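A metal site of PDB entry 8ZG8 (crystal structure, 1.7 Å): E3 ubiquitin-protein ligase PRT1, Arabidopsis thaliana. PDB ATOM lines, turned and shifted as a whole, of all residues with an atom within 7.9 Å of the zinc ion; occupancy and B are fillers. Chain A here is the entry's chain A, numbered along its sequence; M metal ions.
Four residues have an atom within 4 Å of the zinc ion: Cys 9, Cys 12, Cys 36 and Cys 39.
The zinc ion is bound by the side-chain sulfur of Cys 9 (2.3 Å), the side-chain sulfur of Cys 12 (2.3 Å), the side-chain sulfur of Cys 36 (2.3 Å) and the side-chain sulfur of Cys 39 (2.4 Å). The zinc ion has four donor atoms within binding distance.
The side-chain hydroxyl of Ser 11 sits close to the side-chain sulfur of Cys 39 (3.6 Å). SG of Cys 12 sits close to N of Val 14, 3.6 Å away. O of Val 14 is in hydrogen-bond range of N of Cys 9. The backbone NH (N) of Asp 38 lies close to the side-chain sulfur (SG) of Cys 36, 3.7 Å away. The backbone carbonyl oxygen (O) of Cys 39 is in hydrogen-bond range of the side-chain hydroxyl (OG1) of Thr 42 (3.4 Å). N of Ser 11 sits close to SG of Cys 9 (3.4 Å). O of Cys 39 lies within hydrogen-bond range of N of Ser 44, 2.6 Å away.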
ATOM      1  N   GLY A   8       5.432   8.373 -21.224  1.00  0.00           N
ATOM      2  CA  GLY A   8       6.607   7.878 -21.904  1.00  0.00           C
ATOM      3  C   GLY A   8       7.738   7.635 -20.924  1.00  0.00           C
ATOM      4  O   GLY A   8       7.792   8.249 -19.833  1.00  0.00           O
ATOM      5  N   CYS A   9       8.666   6.765 -21.315  1.00  0.00           N
ATOM      6  CA  CYS A   9       9.789   6.414 -20.459  1.00  0.00           C
ATOM      7  C   CYS A   9      10.849   7.528 -20.535  1.00  0.00           C
ATOM      8  O   CYS A   9      11.286   7.838 -21.623  1.00  0.00           O
ATOM      9  CB  CYS A   9      10.441   5.136 -20.914  1.00  0.00           C
ATOM     10  SG  CYS A   9      11.852   4.738 -19.776  1.00  0.00           S
ATOM     11  N   ASP A  10      11.206   8.134 -19.399  1.00  0.00           N
ATOM     12  CA  ASP A  10      12.144   9.261 -19.410  1.00  0.00           C
ATOM     13  C   ASP A  10      13.590   8.796 -19.401  1.00  0.00           C
ATOM     14  O   ASP A  10      14.520   9.652 -19.366  1.00  0.00           O
ATOM     15  CB  ASP A  10      11.858  10.194 -18.216  1.00  0.00           C
ATOM     16  CG  ASP A  10      10.514  10.881 -18.393  1.00  0.00           C
ATOM     17  OD1 ASP A  10      10.303  11.607 -19.356  1.00  0.00           O
ATOM     18  OD2 ASP A  10       9.602  10.708 -17.605  1.00  0.00           O
ATOM     19  N   SER A  11      13.797   7.483 -19.507  1.00  0.00           N
ATOM     20  CA  SER A  11      15.121   6.918 -19.731  1.00  0.00           C
ATOM     21  C   SER A  11      15.328   6.621 -21.207  1.00  0.00           C
ATOM     22  O   SER A  11      16.251   7.130 -21.824  1.00  0.00           O
ATOM     23  CB  SER A  11      15.358   5.638 -18.918  1.00  0.00           C
ATOM     24  OG  SER A  11      16.658   5.191 -19.148  1.00  0.00           O
ATOM     25  N   CYS A  12      14.463   5.779 -21.807  1.00  0.00           N
ATOM     26  CA  CYS A  12      14.643   5.334 -23.185  1.00  0.00           C
ATOM     27  C   CYS A  12      13.706   5.972 -24.197  1.00  0.00           C
ATOM     28  O   CYS A  12      13.903   5.768 -25.413  1.00  0.00           O
ATOM     29  CB  CYS A  12      14.493   3.803 -23.269  1.00  0.00           C
ATOM     30  SG  CYS A  12      12.705   3.200 -23.089  1.00  0.00           S
ATOM     31  N   GLY A  13      12.677   6.690 -23.779  1.00  0.00           N
ATOM     32  CA  GLY A  13      11.829   7.375 -24.751  1.00  0.00           C
ATOM     33  C   GLY A  13      10.683   6.574 -25.343  1.00  0.00           C
ATOM     34  O   GLY A  13       9.984   7.108 -26.218  1.00  0.00           O
ATOM     35  N   VAL A  14      10.456   5.351 -24.871  1.00  0.00           N
ATOM     36  CA  VAL A  14       9.348   4.558 -25.395  1.00  0.00           C
ATOM     37  C   VAL A  14       8.055   5.244 -24.953  1.00  0.00           C
ATOM     38  O   VAL A  14       7.908   5.678 -23.797  1.00  0.00           O
ATOM     39  CB  VAL A  14       9.484   3.103 -24.935  1.00  0.00           C
ATOM     40  CG1 VAL A  14       9.154   2.890 -23.497  1.00  0.00           C
ATOM     41  CG2 VAL A  14       8.665   2.218 -25.853  1.00  0.00           C
ATOM     42  N   TYR A  15       7.137   5.402 -25.897  1.00  0.00           N
ATOM     43  CA  TYR A  15       5.905   6.076 -25.653  1.00  0.00           C
ATOM     44  C   TYR A  15       4.815   5.397 -26.516  1.00  0.00           C
ATOM     45  O   TYR A  15       5.000   5.317 -27.718  1.00  0.00           O
ATOM     46  CB  TYR A  15       5.987   7.578 -26.057  1.00  0.00           C
ATOM     47  CG  TYR A  15       4.628   8.222 -25.853  1.00  0.00           C
ATOM     48  CD1 TYR A  15       4.308   8.736 -24.599  1.00  0.00           C
ATOM     49  CD2 TYR A  15       3.695   8.399 -26.918  1.00  0.00           C
ATOM     50  CE1 TYR A  15       3.093   9.323 -24.373  1.00  0.00           C
ATOM     51  CE2 TYR A  15       2.431   8.957 -26.685  1.00  0.00           C
ATOM     52  CZ  TYR A  15       2.158   9.440 -25.417  1.00  0.00           C
ATOM     53  OH  TYR A  15       0.928   9.985 -25.108  1.00  0.00           O
ATOM     54  N   ILE A  17       4.408   3.729 -22.612  1.00  0.00           N
ATOM     55  CA  ILE A  17       4.959   2.592 -21.907  1.00  0.00           C
ATOM     56  C   ILE A  17       3.982   1.440 -21.969  1.00  0.00           C
ATOM     57  O   ILE A  17       2.795   1.618 -21.668  1.00  0.00           O
ATOM     58  CB  ILE A  17       5.258   2.947 -20.452  1.00  0.00           C
ATOM     59  CG1 ILE A  17       6.389   4.021 -20.448  1.00  0.00           C
ATOM     60  CG2 ILE A  17       5.685   1.721 -19.747  1.00  0.00           C
ATOM     61  CD1 ILE A  17       6.562   4.636 -19.053  1.00  0.00           C
ATOM     62  N   ASP A  34       8.843   9.124 -15.370  1.00  0.00           N
ATOM     63  CA  ASP A  34       8.354   7.752 -15.492  1.00  0.00           C
ATOM     64  C   ASP A  34       9.445   6.880 -16.077  1.00  0.00           C
ATOM     65  O   ASP A  34      10.244   7.366 -16.877  1.00  0.00           O
ATOM     66  CB  ASP A  34       7.179   7.634 -16.482  1.00  0.00           C
ATOM     67  CG  ASP A  34       6.049   8.463 -16.112  1.00  0.00           C
ATOM     68  OD1 ASP A  34       5.322   8.088 -15.169  1.00  0.00           O
ATOM     69  OD2 ASP A  34       5.826   9.468 -16.789  1.00  0.00           O
ATOM     70  N   LEU A  35       9.460   5.599 -15.691  1.00  0.00           N
ATOM     71  CA  LEU A  35      10.323   4.596 -16.290  1.00  0.00           C
ATOM     72  C   LEU A  35       9.546   3.336 -16.693  1.00  0.00           C
ATOM     73  O   LEU A  35       8.667   2.891 -15.953  1.00  0.00           O
ATOM     74  CB  LEU A  35      11.404   4.165 -15.277  1.00  0.00           C
ATOM     75  CG  LEU A  35      12.394   5.280 -14.901  1.00  0.00           C
ATOM     76  CD1 LEU A  35      13.298   4.836 -13.695  1.00  0.00           C
ATOM     77  CD2 LEU A  35      13.252   5.684 -16.140  1.00  0.00           C
ATOM     78  N   CYS A  36       9.924   2.731 -17.831  1.00  0.00           N
ATOM     79  CA  CYS A  36       9.455   1.392 -18.198  1.00  0.00           C
ATOM     80  C   CYS A  36      10.179   0.313 -17.378  1.00  0.00           C
ATOM     81  O   CYS A  36      11.190   0.541 -16.669  1.00  0.00           O
ATOM     82  CB  CYS A  36       9.672   1.154 -19.715  1.00  0.00           C
ATOM     83  SG  CYS A  36      11.436   0.870 -20.217  1.00  0.00           S
ATOM     84  N   LYS A  37       9.670  -0.916 -17.491  1.00  0.00           N
ATOM     85  CA  LYS A  37      10.208  -1.974 -16.662  1.00  0.00           C
ATOM     86  C   LYS A  37      11.662  -2.209 -16.971  1.00  0.00           C
ATOM     87  O   LYS A  37      12.452  -2.432 -16.046  1.00  0.00           O
ATOM     88  CB  LYS A  37       9.431  -3.295 -16.829  1.00  0.00           C
ATOM     89  CG  LYS A  37       9.995  -4.331 -15.978  1.00  0.00           C
ATOM     90  CD  LYS A  37       9.355  -5.745 -16.067  1.00  0.00           C
ATOM     91  CE  LYS A  37       9.955  -6.322 -17.458  1.00  0.00           C
ATOM     92  NZ  LYS A  37       9.657  -7.856 -17.458  1.00  0.00           N
ATOM     93  N   ASP A  38      12.030  -2.216 -18.258  1.00  0.00           N
ATOM     94  CA  ASP A  38      13.428  -2.485 -18.647  1.00  0.00           C
ATOM     95  C   ASP A  38      14.399  -1.445 -18.114  1.00  0.00           C
ATOM     96  O   ASP A  38      15.477  -1.798 -17.616  1.00  0.00           O
ATOM     97  CB  ASP A  38      13.564  -2.549 -20.166  1.00  0.00           C
ATOM     98  CG  ASP A  38      12.883  -3.768 -20.773  1.00  0.00           C
ATOM     99  OD1 ASP A  38      12.652  -4.749 -20.015  1.00  0.00           O
ATOM    100  OD2 ASP A  38      12.617  -3.763 -21.999  1.00  0.00           O
ATOM    101  N   CYS A  39      14.028  -0.187 -18.173  1.00  0.00           N
ATOM    102  CA  CYS A  39      14.869   0.887 -17.663  1.00  0.00           C
ATOM    103  C   CYS A  39      14.877   0.847 -16.151  1.00  0.00           C
ATOM    104  O   CYS A  39      15.894   1.144 -15.536  1.00  0.00           O
ATOM    105  CB  CYS A  39      14.412   2.222 -18.217  1.00  0.00           C
ATOM    106  SG  CYS A  39      14.711   2.253 -20.019  1.00  0.00           S
ATOM    107  N   TYR A  40      13.729   0.567 -15.526  1.00  0.00           N
ATOM    108  CA  TYR A  40      13.744   0.610 -14.074  1.00  0.00           C
ATOM    109  C   TYR A  40      14.587  -0.519 -13.483  1.00  0.00           C
ATOM    110  O   TYR A  40      15.305  -0.282 -12.487  1.00  0.00           O
ATOM    111  CB  TYR A  40      12.300   0.532 -13.494  1.00  0.00           C
ATOM    112  CG  TYR A  40      12.181   0.400 -11.969  1.00  0.00           C
ATOM    113  CD1 TYR A  40      12.110   1.561 -11.198  1.00  0.00           C
ATOM    114  CD2 TYR A  40      12.037  -0.841 -11.308  1.00  0.00           C
ATOM    115  CE1 TYR A  40      11.994   1.511  -9.833  1.00  0.00           C
ATOM    116  CE2 TYR A  40      11.879  -0.911  -9.908  1.00  0.00           C
ATOM    117  CZ  TYR A  40      11.849   0.278  -9.178  1.00  0.00           C
ATOM    118  OH  TYR A  40      11.712   0.264  -7.810  1.00  0.00           O
ATOM    119  N   THR A  42      17.467  -1.796 -14.533  1.00  0.00           N
ATOM    120  CA  THR A  42      18.870  -1.709 -14.925  1.00  0.00           C
ATOM    121  C   THR A  42      19.463  -0.384 -14.439  1.00  0.00           C
ATOM    122  O   THR A  42      19.118   0.089 -13.349  1.00  0.00           O
ATOM    123  CB  THR A  42      19.019  -1.790 -16.452  1.00  0.00           C
ATOM    124  OG1 THR A  42      18.301  -0.694 -17.036  1.00  0.00           O
ATOM    125  CG2 THR A  42      18.415  -3.104 -16.953  1.00  0.00           C
ATOM    126  N   SER A  44      17.614   2.645 -14.372  1.00  0.00           N
ATOM    127  CA  SER A  44      17.445   3.940 -15.000  1.00  0.00           C
ATOM    128  C   SER A  44      18.626   4.059 -15.910  1.00  0.00           C
ATOM    129  O   SER A  44      19.156   3.021 -16.354  1.00  0.00           O
ATOM    130  CB  SER A  44      17.419   5.065 -13.988  1.00  0.00           C
ATOM    131  OG  SER A  44      16.828   6.210 -14.589  1.00  0.00           O
ATOM    132  N   LYS A  45      19.071   5.315 -16.146  1.00  0.00           N
ATOM    133  CA  LYS A  45      20.210   5.545 -17.016  1.00  0.00           C
ATOM    134  C   LYS A  45      21.387   6.353 -16.390  1.00  0.00           C
ATOM    135  O   LYS A  45      21.196   7.224 -15.550  1.00  0.00           O
ATOM    136  CB  LYS A  45      19.823   6.305 -18.307  1.00  0.00           C
ATOM    137  CG  LYS A  45      19.448   5.429 -19.376  1.00  0.00           C
ATOM    138  CD  LYS A  45      20.735   4.810 -19.779  1.00  0.00           C
ATOM    139  CE  LYS A  45      20.504   3.509 -20.391  1.00  0.00           C
ATOM    140  NZ  LYS A  45      19.490   3.568 -21.491  1.00  0.00           N
HETATM  141 ZN    ZN M   1      12.564   2.831 -20.802  1.00  0.00          ZN
